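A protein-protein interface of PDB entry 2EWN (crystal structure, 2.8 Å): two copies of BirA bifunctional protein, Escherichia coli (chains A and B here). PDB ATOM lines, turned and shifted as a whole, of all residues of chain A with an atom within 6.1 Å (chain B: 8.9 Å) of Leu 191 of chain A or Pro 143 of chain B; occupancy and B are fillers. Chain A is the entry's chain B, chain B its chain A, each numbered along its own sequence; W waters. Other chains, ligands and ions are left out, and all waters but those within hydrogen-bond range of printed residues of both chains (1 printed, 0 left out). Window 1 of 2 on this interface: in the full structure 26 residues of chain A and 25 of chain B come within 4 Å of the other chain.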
ATOM      1  N   LEU A  95       9.978  14.616 -21.322  1.00  0.00           N
ATOM      2  CA  LEU A  95      10.522  15.572 -20.377  1.00  0.00           C
ATOM      3  C   LEU A  95      11.527  16.464 -21.088  1.00  0.00           C
ATOM      4  O   LEU A  95      11.610  17.663 -20.827  1.00  0.00           O
ATOM      5  CB  LEU A  95      11.208  14.846 -19.225  1.00  0.00           C
ATOM      6  CG  LEU A  95      10.273  14.325 -18.135  1.00  0.00           C
ATOM      7  CD1 LEU A  95      11.084  13.671 -17.039  1.00  0.00           C
ATOM      8  CD2 LEU A  95       9.464  15.479 -17.562  1.00  0.00           C
ATOM      9  N   GLY A 142      -1.946  24.010 -11.762  1.00  0.00           N
ATOM     10  CA  GLY A 142      -0.719  23.676 -11.048  1.00  0.00           C
ATOM     11  C   GLY A 142      -0.556  22.334 -10.341  1.00  0.00           C
ATOM     12  O   GLY A 142      -1.375  21.419 -10.529  1.00  0.00           O
ATOM     13  N   PRO A 143       0.505  22.231  -9.535  1.00  0.00           N
ATOM     14  CA  PRO A 143       0.852  21.018  -8.787  1.00  0.00           C
ATOM     15  C   PRO A 143      -0.180  20.474  -7.813  1.00  0.00           C
ATOM     16  O   PRO A 143      -0.232  19.268  -7.576  1.00  0.00           O
ATOM     17  CB  PRO A 143       2.147  21.409  -8.059  1.00  0.00           C
ATOM     18  CG  PRO A 143       2.639  22.691  -8.820  1.00  0.00           C
ATOM     19  CD  PRO A 143       1.342  23.371  -9.113  1.00  0.00           C
ATOM     20  N   ALA A 144      -0.997  21.342  -7.226  1.00  0.00           N
ATOM     21  CA  ALA A 144      -1.992  20.890  -6.267  1.00  0.00           C
ATOM     22  C   ALA A 144      -2.905  19.874  -6.929  1.00  0.00           C
ATOM     23  O   ALA A 144      -3.448  18.969  -6.283  1.00  0.00           O
ATOM     24  CB  ALA A 144      -2.794  22.069  -5.761  1.00  0.00           C
ATOM     25  N   ALA A 146      -1.950  17.640  -9.285  1.00  0.00           N
ATOM     26  CA  ALA A 146      -1.277  16.448  -9.800  1.00  0.00           C
ATOM     27  C   ALA A 146      -1.823  15.098  -9.334  1.00  0.00           C
ATOM     28  O   ALA A 146      -1.978  14.180 -10.136  1.00  0.00           O
ATOM     29  CB  ALA A 146       0.199  16.521  -9.503  1.00  0.00           C
ATOM     30  N   ILE A 147      -2.093  14.970  -8.042  1.00  0.00           N
ATOM     31  CA  ILE A 147      -2.597  13.721  -7.487  1.00  0.00           C
ATOM     32  C   ILE A 147      -3.954  13.357  -8.102  1.00  0.00           C
ATOM     33  O   ILE A 147      -4.142  12.244  -8.581  1.00  0.00           O
ATOM     34  CB  ILE A 147      -2.704  13.834  -5.946  1.00  0.00           C
ATOM     35  CG1 ILE A 147      -2.136  12.579  -5.277  1.00  0.00           C
ATOM     36  CG2 ILE A 147      -4.133  14.117  -5.529  1.00  0.00           C
ATOM     37  CD1 ILE A 147      -0.636  12.660  -4.987  1.00  0.00           C
ATOM     38  N   VAL A 189       3.795   9.252 -13.186  1.00  0.00           N
ATOM     39  CA  VAL A 189       3.517  10.663 -13.473  1.00  0.00           C
ATOM     40  C   VAL A 189       4.654  11.535 -12.949  1.00  0.00           C
ATOM     41  O   VAL A 189       4.885  11.598 -11.747  1.00  0.00           O
ATOM     42  CB  VAL A 189       2.206  11.142 -12.772  1.00  0.00           C
ATOM     43  CG1 VAL A 189       1.984  12.631 -13.029  1.00  0.00           C
ATOM     44  CG2 VAL A 189       1.014  10.346 -13.270  1.00  0.00           C
ATOM     45  N   GLU A 190       5.370  12.199 -13.843  1.00  0.00           N
ATOM     46  CA  GLU A 190       6.461  13.077 -13.433  1.00  0.00           C
ATOM     47  C   GLU A 190       6.016  14.528 -13.763  1.00  0.00           C
ATOM     48  O   GLU A 190       5.173  14.727 -14.640  1.00  0.00           O
ATOM     49  CB  GLU A 190       7.772  12.714 -14.149  1.00  0.00           C
ATOM     50  CG  GLU A 190       8.202  11.256 -13.983  1.00  0.00           C
ATOM     51  CD  GLU A 190       9.525  10.907 -14.651  1.00  0.00           C
ATOM     52  OE1 GLU A 190      10.585  11.343 -14.159  1.00  0.00           O
ATOM     53  OE2 GLU A 190       9.506  10.194 -15.672  1.00  0.00           O
ATOM     54  N   LEU A 191       6.578  15.540 -13.086  1.00  0.00           N
ATOM     55  CA  LEU A 191       6.142  16.912 -13.378  1.00  0.00           C
ATOM     56  C   LEU A 191       7.139  18.026 -12.976  1.00  0.00           C
ATOM     57  O   LEU A 191       7.999  17.831 -12.128  1.00  0.00           O
ATOM     58  CB  LEU A 191       4.838  17.190 -12.631  1.00  0.00           C
ATOM     59  CG  LEU A 191       4.953  17.374 -11.114  1.00  0.00           C
ATOM     60  CD1 LEU A 191       4.234  18.647 -10.671  1.00  0.00           C
ATOM     61  CD2 LEU A 191       4.391  16.168 -10.368  1.00  0.00           C
ATOM     62  N   THR A 192       7.007  19.215 -13.620  1.00  0.00           N
ATOM     63  CA  THR A 192       7.749  20.488 -13.303  1.00  0.00           C
ATOM     64  C   THR A 192       6.669  21.562 -13.280  1.00  0.00           C
ATOM     65  O   THR A 192       5.869  21.634 -14.220  1.00  0.00           O
ATOM     66  CB  THR A 192       8.817  20.926 -14.315  1.00  0.00           C
ATOM     67  OG1 THR A 192       8.184  21.228 -15.559  1.00  0.00           O
ATOM     68  CG2 THR A 192       9.845  19.832 -14.506  1.00  0.00           C
ATOM     69  N   GLY A 193       6.634  22.399 -12.237  1.00  0.00           N
ATOM     70  CA  GLY A 193       5.633  23.452 -12.168  1.00  0.00           C
ATOM     71  C   GLY A 193       6.042  24.522 -11.181  1.00  0.00           C
ATOM     72  O   GLY A 193       7.069  24.437 -10.532  1.00  0.00           O
ATOM     73  N   ALA A 199       1.518  23.494 -14.170  1.00  0.00           N
ATOM     74  CA  ALA A 199       2.393  22.357 -13.949  1.00  0.00           C
ATOM     75  C   ALA A 199       2.513  21.617 -15.278  1.00  0.00           C
ATOM     76  O   ALA A 199       1.493  21.403 -15.948  1.00  0.00           O
ATOM     77  CB  ALA A 199       1.788  21.443 -12.903  1.00  0.00           C
ATOM     78  N   GLN A 200       3.737  21.261 -15.683  1.00  0.00           N
ATOM     79  CA  GLN A 200       3.951  20.487 -16.915  1.00  0.00           C
ATOM     80  C   GLN A 200       4.043  19.040 -16.482  1.00  0.00           C
ATOM     81  O   GLN A 200       4.896  18.667 -15.678  1.00  0.00           O
ATOM     82  CB  GLN A 200       5.244  20.876 -17.629  1.00  0.00           C
ATOM     83  CG  GLN A 200       5.167  22.230 -18.292  1.00  0.00           C
ATOM     84  CD  GLN A 200       5.190  23.327 -17.273  1.00  0.00           C
ATOM     85  OE1 GLN A 200       4.368  24.243 -17.306  1.00  0.00           O
ATOM     86  NE2 GLN A 200       6.138  23.246 -16.346  1.00  0.00           N
ATOM     87  N   ILE A 201       3.158  18.224 -17.019  1.00  0.00           N
ATOM     88  CA  ILE A 201       3.120  16.850 -16.609  1.00  0.00           C
ATOM     89  C   ILE A 201       3.374  15.832 -17.700  1.00  0.00           C
ATOM     90  O   ILE A 201       2.949  15.999 -18.843  1.00  0.00           O
ATOM     91  CB  ILE A 201       1.785  16.609 -15.888  1.00  0.00           C
ATOM     92  CG1 ILE A 201       1.803  17.424 -14.595  1.00  0.00           C
ATOM     93  CG2 ILE A 201       1.556  15.127 -15.597  1.00  0.00           C
ATOM     94  CD1 ILE A 201       0.452  17.694 -14.014  1.00  0.00           C
ATOM     95  N   VAL A 202       4.115  14.789 -17.331  1.00  0.00           N
ATOM     96  CA  VAL A 202       4.436  13.688 -18.231  1.00  0.00           C
ATOM     97  C   VAL A 202       3.938  12.428 -17.565  1.00  0.00           C
ATOM     98  O   VAL A 202       4.357  12.062 -16.465  1.00  0.00           O
ATOM     99  CB  VAL A 202       5.938  13.542 -18.482  1.00  0.00           C
ATOM    100  CG1 VAL A 202       6.196  12.213 -19.145  1.00  0.00           C
ATOM    101  CG2 VAL A 202       6.433  14.674 -19.389  1.00  0.00           C
ATOM    102  N   LEU B  95      18.080  24.546  -9.195  1.00  0.00           N
ATOM    103  CA  LEU B  95      17.383  23.549 -10.017  1.00  0.00           C
ATOM    104  C   LEU B  95      18.368  22.697 -10.813  1.00  0.00           C
ATOM    105  O   LEU B  95      18.136  21.502 -11.035  1.00  0.00           O
ATOM    106  CB  LEU B  95      16.407  24.237 -10.968  1.00  0.00           C
ATOM    107  CG  LEU B  95      15.025  24.580 -10.406  1.00  0.00           C
ATOM    108  CD1 LEU B  95      14.262  25.320 -11.481  1.00  0.00           C
ATOM    109  CD2 LEU B  95      14.271  23.323  -9.989  1.00  0.00           C
ATOM    110  N   ILE B  98      19.962  19.932  -8.247  1.00  0.00           N
ATOM    111  CA  ILE B  98      19.053  19.104  -7.466  1.00  0.00           C
ATOM    112  C   ILE B  98      19.659  17.791  -6.942  1.00  0.00           C
ATOM    113  O   ILE B  98      19.318  17.333  -5.841  1.00  0.00           O
ATOM    114  CB  ILE B  98      17.786  18.812  -8.312  1.00  0.00           C
ATOM    115  CG1 ILE B  98      16.845  20.005  -8.235  1.00  0.00           C
ATOM    116  CG2 ILE B  98      17.094  17.531  -7.860  1.00  0.00           C
ATOM    117  CD1 ILE B  98      15.597  19.817  -9.056  1.00  0.00           C
ATOM    118  N   LEU B 139      10.939  17.400  -0.100  1.00  0.00           N
ATOM    119  CA  LEU B 139       9.677  17.011   0.540  1.00  0.00           C
ATOM    120  C   LEU B 139       9.304  15.576   0.260  1.00  0.00           C
ATOM    121  O   LEU B 139       9.004  15.237  -0.881  1.00  0.00           O
ATOM    122  CB  LEU B 139       8.520  17.833  -0.008  1.00  0.00           C
ATOM    123  CG  LEU B 139       8.092  19.137   0.629  1.00  0.00           C
ATOM    124  CD1 LEU B 139       6.733  19.522   0.042  1.00  0.00           C
ATOM    125  CD2 LEU B 139       8.005  18.971   2.141  1.00  0.00           C
ATOM    126  N   GLU B 140       9.253  14.738   1.281  1.00  0.00           N
ATOM    127  CA  GLU B 140       8.896  13.347   1.037  1.00  0.00           C
ATOM    128  C   GLU B 140       7.414  13.148   0.699  1.00  0.00           C
ATOM    129  O   GLU B 140       7.043  12.126   0.130  1.00  0.00           O
ATOM    130  CB  GLU B 140       9.299  12.485   2.235  1.00  0.00           C
ATOM    131  CG  GLU B 140      10.805  12.223   2.322  1.00  0.00           C
ATOM    132  CD  GLU B 140      11.334  11.448   1.112  1.00  0.00           C
ATOM    133  OE1 GLU B 140      10.533  10.710   0.487  1.00  0.00           O
ATOM    134  OE2 GLU B 140      12.543  11.565   0.792  1.00  0.00           O
ATOM    135  N   GLN B 141       6.578  14.131   1.030  1.00  0.00           N
ATOM    136  CA  GLN B 141       5.142  14.056   0.765  1.00  0.00           C
ATOM    137  C   GLN B 141       4.816  14.234  -0.701  1.00  0.00           C
ATOM    138  O   GLN B 141       3.679  13.999  -1.116  1.00  0.00           O
ATOM    139  CB  GLN B 141       4.368  15.123   1.554  1.00  0.00           C
ATOM    140  CG  GLN B 141       4.261  14.838   3.032  1.00  0.00           C
ATOM    141  CD  GLN B 141       5.086  15.806   3.857  1.00  0.00           C
ATOM    142  OE1 GLN B 141       4.663  16.947   4.121  1.00  0.00           O
ATOM    143  NE2 GLN B 141       6.282  15.366   4.255  1.00  0.00           N
ATOM    144  N   GLY B 142       5.796  14.671  -1.486  1.00  0.00           N
ATOM    145  CA  GLY B 142       5.562  14.841  -2.909  1.00  0.00           C
ATOM    146  C   GLY B 142       4.878  16.130  -3.314  1.00  0.00           C
ATOM    147  O   GLY B 142       4.749  17.036  -2.493  1.00  0.00           O
ATOM    148  N   PRO B 143       4.395  16.229  -4.569  1.00  0.00           N
ATOM    149  CA  PRO B 143       3.722  17.399  -5.172  1.00  0.00           C
ATOM    150  C   PRO B 143       2.505  17.990  -4.428  1.00  0.00           C
ATOM    151  O   PRO B 143       2.253  19.191  -4.490  1.00  0.00           O
ATOM    152  CB  PRO B 143       3.327  16.905  -6.576  1.00  0.00           C
ATOM    153  CG  PRO B 143       4.277  15.766  -6.837  1.00  0.00           C
ATOM    154  CD  PRO B 143       4.320  15.084  -5.494  1.00  0.00           C
ATOM    155  N   ALA B 144       1.733  17.163  -3.731  1.00  0.00           N
ATOM    156  CA  ALA B 144       0.565  17.644  -3.006  1.00  0.00           C
ATOM    157  C   ALA B 144       0.885  18.742  -1.982  1.00  0.00           C
ATOM    158  O   ALA B 144       0.146  19.729  -1.825  1.00  0.00           O
ATOM    159  CB  ALA B 144      -0.115  16.467  -2.310  1.00  0.00           C
ATOM    160  N   ALA B 145       2.010  18.569  -1.299  1.00  0.00           N
ATOM    161  CA  ALA B 145       2.469  19.489  -0.262  1.00  0.00           C
ATOM    162  C   ALA B 145       3.087  20.815  -0.721  1.00  0.00           C
ATOM    163  O   ALA B 145       3.414  21.655   0.108  1.00  0.00           O
ATOM    164  CB  ALA B 145       3.445  18.766   0.623  1.00  0.00           C
ATOM    165  N   ALA B 146       3.259  21.011  -2.024  1.00  0.00           N
ATOM    166  CA  ALA B 146       3.866  22.241  -2.520  1.00  0.00           C
ATOM    167  C   ALA B 146       3.065  23.508  -2.231  1.00  0.00           C
ATOM    168  O   ALA B 146       3.643  24.543  -1.883  1.00  0.00           O
ATOM    169  CB  ALA B 146       4.119  22.141  -4.009  1.00  0.00           C
ATOM    170  N   ILE B 147       1.744  23.451  -2.381  1.00  0.00           N
ATOM    171  CA  ILE B 147       0.972  24.653  -2.119  1.00  0.00           C
ATOM    172  C   ILE B 147       1.105  24.995  -0.635  1.00  0.00           C
ATOM    173  O   ILE B 147       1.294  26.157  -0.284  1.00  0.00           O
ATOM    174  CB  ILE B 147      -0.507  24.487  -2.534  1.00  0.00           C
ATOM    175  CG1 ILE B 147      -0.993  25.760  -3.240  1.00  0.00           C
ATOM    176  CG2 ILE B 147      -1.367  24.184  -1.327  1.00  0.00           C
ATOM    177  CD1 ILE B 147      -0.484  25.898  -4.666  1.00  0.00           C
ATOM    178  N   GLY B 148       1.037  23.986   0.231  1.00  0.00           N
ATOM    179  CA  GLY B 148       1.189  24.248   1.648  1.00  0.00           C
ATOM    180  C   GLY B 148       2.540  24.898   1.913  1.00  0.00           C
ATOM    181  O   GLY B 148       2.650  25.848   2.672  1.00  0.00           O
ATOM    182  N   LEU B 149       3.584  24.386   1.283  1.00  0.00           N
ATOM    183  CA  LEU B 149       4.911  24.939   1.473  1.00  0.00           C
ATOM    184  C   LEU B 149       4.920  26.421   1.129  1.00  0.00           C
ATOM    185  O   LEU B 149       5.488  27.207   1.870  1.00  0.00           O
ATOM    186  CB  LEU B 149       5.922  24.177   0.622  1.00  0.00           C
ATOM    187  CG  LEU B 149       7.385  24.542   0.829  1.00  0.00           C
ATOM    188  CD1 LEU B 149       8.239  23.283   0.909  1.00  0.00           C
ATOM    189  CD2 LEU B 149       7.817  25.434  -0.320  1.00  0.00           C
ATOM    190  N   GLU B 190       9.448  26.661  -7.333  1.00  0.00           N
ATOM    191  CA  GLU B 190       9.385  25.756  -8.477  1.00  0.00           C
ATOM    192  C   GLU B 190       9.652  24.335  -7.984  1.00  0.00           C
ATOM    193  O   GLU B 190      10.275  24.142  -6.940  1.00  0.00           O
ATOM    194  CB  GLU B 190      10.417  26.141  -9.538  1.00  0.00           C
ATOM    195  CG  GLU B 190      10.822  27.618  -9.543  1.00  0.00           C
ATOM    196  CD  GLU B 190      11.509  28.064 -10.844  1.00  0.00           C
ATOM    197  OE1 GLU B 190      11.184  27.507 -11.912  1.00  0.00           O
ATOM    198  OE2 GLU B 190      12.382  28.964 -10.791  1.00  0.00           O
ATOM    199  N   LEU B 191       9.184  23.331  -8.713  1.00  0.00           N
ATOM    200  CA  LEU B 191       9.454  21.971  -8.263  1.00  0.00           C
ATOM    201  C   LEU B 191       9.402  20.901  -9.376  1.00  0.00           C
ATOM    202  O   LEU B 191       8.850  21.097 -10.461  1.00  0.00           O
ATOM    203  CB  LEU B 191       8.434  21.537  -7.195  1.00  0.00           C
ATOM    204  CG  LEU B 191       7.147  20.920  -7.751  1.00  0.00           C
ATOM    205  CD1 LEU B 191       6.322  20.283  -6.644  1.00  0.00           C
ATOM    206  CD2 LEU B 191       6.325  21.981  -8.476  1.00  0.00           C
ATOM    207  N   THR B 192      10.052  19.774  -9.075  1.00  0.00           N
ATOM    208  CA  THR B 192      10.072  18.593  -9.902  1.00  0.00           C
ATOM    209  C   THR B 192       9.717  17.499  -8.932  1.00  0.00           C
ATOM    210  O   THR B 192      10.087  17.577  -7.765  1.00  0.00           O
ATOM    211  CB  THR B 192      11.438  18.269 -10.514  1.00  0.00           C
ATOM    212  OG1 THR B 192      12.429  18.225  -9.472  1.00  0.00           O
ATOM    213  CG2 THR B 192      11.825  19.333 -11.550  1.00  0.00           C
ATOM    214  N   GLY B 193       9.006  16.484  -9.381  1.00  0.00           N
ATOM    215  CA  GLY B 193       8.652  15.399  -8.489  1.00  0.00           C
ATOM    216  C   GLY B 193       7.848  14.400  -9.279  1.00  0.00           C
ATOM    217  O   GLY B 193       7.706  14.543 -10.505  1.00  0.00           O
ATOM    218  N   LYS B 194       7.326  13.396  -8.613  1.00  0.00           N
ATOM    219  CA  LYS B 194       6.474  12.386  -9.238  1.00  0.00           C
ATOM    220  C   LYS B 194       5.436  12.008  -8.204  1.00  0.00           C
ATOM    221  O   LYS B 194       5.783  11.758  -7.045  1.00  0.00           O
ATOM    222  CB  LYS B 194       7.296  11.184  -9.688  1.00  0.00           C
ATOM    223  CG  LYS B 194       8.801  11.345  -9.455  1.00  0.00           C
ATOM    224  CD  LYS B 194       9.518  10.007  -9.463  1.00  0.00           C
ATOM    225  CE  LYS B 194      10.215   9.755 -10.774  1.00  0.00           C
ATOM    226  NZ  LYS B 194      11.453  10.570 -10.903  1.00  0.00           N
ATOM    227  N   THR B 195       4.169  11.955  -8.595  1.00  0.00           N
ATOM    228  CA  THR B 195       3.151  11.602  -7.624  1.00  0.00           C
ATOM    229  C   THR B 195       3.488  10.218  -7.069  1.00  0.00           C
ATOM    230  O   THR B 195       3.792   9.299  -7.828  1.00  0.00           O
ATOM    231  CB  THR B 195       1.745  11.639  -8.245  1.00  0.00           C
ATOM    232  OG1 THR B 195       1.676  10.697  -9.321  1.00  0.00           O
ATOM    233  CG2 THR B 195       1.433  13.040  -8.784  1.00  0.00           C
ATOM    234  N   GLY B 196       3.488  10.105  -5.739  1.00  0.00           N
ATOM    235  CA  GLY B 196       3.810   8.864  -5.053  1.00  0.00           C
ATOM    236  C   GLY B 196       5.285   8.740  -4.679  1.00  0.00           C
ATOM    237  O   GLY B 196       5.754   7.677  -4.261  1.00  0.00           O
ATOM    238  N   ASP B 197       6.032   9.827  -4.821  1.00  0.00           N
ATOM    239  CA  ASP B 197       7.460   9.816  -4.516  1.00  0.00           C
ATOM    240  C   ASP B 197       7.785  11.210  -3.967  1.00  0.00           C
ATOM    241  O   ASP B 197       6.874  12.008  -3.742  1.00  0.00           O
ATOM    242  CB  ASP B 197       8.208   9.510  -5.824  1.00  0.00           C
ATOM    243  CG  ASP B 197       9.645   9.097  -5.617  1.00  0.00           C
ATOM    244  OD1 ASP B 197      10.188   8.477  -6.559  1.00  0.00           O
ATOM    245  OD2 ASP B 197      10.231   9.395  -4.551  1.00  0.00           O
ATOM    246  N   ALA B 198       9.055  11.512  -3.738  1.00  0.00           N
ATOM    247  CA  ALA B 198       9.425  12.830  -3.237  1.00  0.00           C
ATOM    248  C   ALA B 198       9.250  13.980  -4.242  1.00  0.00           C
ATOM    249  O   ALA B 198       8.922  13.799  -5.421  1.00  0.00           O
ATOM    250  CB  ALA B 198      10.863  12.807  -2.740  1.00  0.00           C
ATOM    251  N   ALA B 199       9.471  15.184  -3.742  1.00  0.00           N
ATOM    252  CA  ALA B 199       9.383  16.371  -4.561  1.00  0.00           C
ATOM    253  C   ALA B 199      10.624  17.174  -4.216  1.00  0.00           C
ATOM    254  O   ALA B 199      11.033  17.247  -3.049  1.00  0.00           O
ATOM    255  CB  ALA B 199       8.121  17.157  -4.226  1.00  0.00           C
ATOM    256  N   GLN B 200      11.262  17.716  -5.245  1.00  0.00           N
ATOM    257  CA  GLN B 200      12.439  18.540  -5.059  1.00  0.00           C
ATOM    258  C   GLN B 200      11.949  19.951  -5.298  1.00  0.00           C
ATOM    259  O   GLN B 200      11.490  20.293  -6.386  1.00  0.00           O
ATOM    260  CB  GLN B 200      13.534  18.172  -6.058  1.00  0.00           C
ATOM    261  CG  GLN B 200      14.238  16.871  -5.746  1.00  0.00           C
ATOM    262  CD  GLN B 200      13.396  15.677  -6.108  1.00  0.00           C
ATOM    263  OE1 GLN B 200      13.448  14.648  -5.428  1.00  0.00           O
ATOM    264  NE2 GLN B 200      12.616  15.794  -7.192  1.00  0.00           N
ATOM    265  N   ILE B 201      12.060  20.772  -4.268  1.00  0.00           N
ATOM    266  CA  ILE B 201      11.563  22.127  -4.337  1.00  0.00           C
ATOM    267  C   ILE B 201      12.608  23.219  -4.217  1.00  0.00           C
ATOM    268  O   ILE B 201      13.525  23.123  -3.410  1.00  0.00           O
ATOM    269  CB  ILE B 201      10.502  22.261  -3.260  1.00  0.00           C
ATOM    270  CG1 ILE B 201       9.373  21.301  -3.604  1.00  0.00           C
ATOM    271  CG2 ILE B 201      10.015  23.679  -3.148  1.00  0.00           C
ATOM    272  CD1 ILE B 201       8.463  20.990  -2.465  1.00  0.00           C
ATOM    273  N   PHE B 253       6.944  22.142   9.080  1.00  0.00           N
ATOM    274  CA  PHE B 253       5.947  21.823   8.046  1.00  0.00           C
ATOM    275  C   PHE B 253       6.025  20.359   7.583  1.00  0.00           C
ATOM    276  O   PHE B 253       5.008  19.667   7.424  1.00  0.00           O
ATOM    277  CB  PHE B 253       6.173  22.732   6.832  1.00  0.00           C
ATOM    278  CG  PHE B 253       5.281  22.417   5.673  1.00  0.00           C
ATOM    279  CD1 PHE B 253       3.918  22.666   5.740  1.00  0.00           C
ATOM    280  CD2 PHE B 253       5.794  21.806   4.540  1.00  0.00           C
ATOM    281  CE1 PHE B 253       3.081  22.306   4.696  1.00  0.00           C
ATOM    282  CE2 PHE B 253       4.960  21.445   3.484  1.00  0.00           C
ATOM    283  CZ  PHE B 253       3.601  21.693   3.567  1.00  0.00           C
HETATM  284  O   HOH W   1       4.278   8.531 -10.369  1.00  0.00           O
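The backbone carbonyl oxygen (O) of Thr 192 of chain B is in hydrogen-bond range of the backbone NH (N) of Gln 200 of chain B, at 2.8 Å. The backbone NH (N) of Glu 190 of chain A sits at hydrogen-bond distance from the backbone carbonyl oxygen (O) of Val 202 of chain A (2.8 Å). O of Thr 192 of chain A lies within hydrogen-bond range of N of Gln 200 of chain A, at 2.6 Å.
The backbone carbonyl oxygen (O) of Gly 193 of chain A is in hydrogen-bond range of the backbone NH (N) of Leu 191 of chain B (3.0 Å). The backbone NH (N) of Leu 191 of chain A lies within hydrogen-bond range of the backbone carbonyl oxygen (O) of Gly 193 of chain B, at 3.0 Å. The side-chain amino group of Lys 194 of chain B lies within salt-bridge range of the side-chain carboxylate of Glu 190 of chain A (3.5 Å). The backbone NH of Thr 195 of chain B lies within hydrogen-bond range of the backbone carbonyl oxygen of Val 189 of chain A (3.3 Å).
Water W1 lies within hydrogen-bond range of O of Thr 195 of chain B and N of Val 189 of chain A.
Among the printed residues, merely in contact across the chains: Val 189 of chain A with Lys 194 of chain B (3.1 Å), Thr 192 of chain A with Leu 191 of chain B (3.1 Å), Leu 191 of chain A with Thr 192 of chain B (3.1 Å), Gly 193 of chain A with Glu 190 of chain B (3.4 Å), Glu 190 of chain A with Gly 193 of chain B (3.5 Å), Leu 191 of chain A with Pro 143 of chain B (3.6 Å), Thr 192 of chain A with Thr 192 of chain B (3.6 Å), Ala 146 of chain A with Thr 195 of chain B (3.8 Å), Leu 191 of chain A with Leu 191 of chain B (3.8 Å), Pro 143 of chain A with Leu 191 of chain B (3.8 Å) and Pro 143 of chain A with Pro 143 of chain B (3.96 Å).
Leu 191 of chain A touches just these residues of chain B: Pro 143 (3.6 Å), Leu 191 (3.8 Å), Thr 192 (3.1 Å) and Gly 193 (3.0 Å). Pro 143 of chain B touches two residues of chain A. Thr 192 of chain A touches just these residues of chain B: Leu 191 and Thr 192. Of the printed residues of chain A, Leu 191 of chain B touches Pro 143 (3.8 Å), Leu 191 (3.8 Å), Thr 192 (3.1 Å) and Gly 193 (3.0 Å). Printed residues of chain B within 4 Å of Pro 143 of chain A: Pro 143 (3.96 Å) and Leu 191 (3.8 Å). Printed residues of chain A within 4 Å of Thr 192 of chain B: Leu 191 (3.1 Å) and Thr 192 (3.6 Å). Of the printed residues of chain B, Gly 193 of chain A touches Glu 190 (3.4 Å) and Leu 191 (3.0 Å). Printed residues of chain A within 4 Å of Glu 190 of chain B: Gly 193 (3.4 Å). The nearest residue of chain A that does not touch Pro 143 of chain B is Ala 146 of chain A (4.3 Å).
Of the 26 printed residues of chain B, 7 touch a printed residue of chain A. Hydrophobic or aromatic side chains of chain B that line the printed part of chain A: Pro 143 and Leu 191. Among the printed residues, Asp or Glu carboxylates within 4 Å of a Lys or Arg side-chain nitrogen of the other chain: Glu 190 of chain A with Lys 194 of chain B.
Pro 143 of chain B touches its own counterpart, Pro 143 of chain A. Pro 143 of chain A touches Leu 191 of chain B, and with the chains exchanged Leu 191 of chain A touches Pro 143 of chain B. Leu 191 of chain A touches Gly 193 of chain B, and with the chains exchanged Gly 193 of chain A touches Leu 191 of chain B. Thr 192 of chain B touches its own counterpart, Thr 192 of chain A. Positions printed for both chains: 95, 142, 143, 144, 146, 147, 190, 191, 192, 193, 199, 200 and 201.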
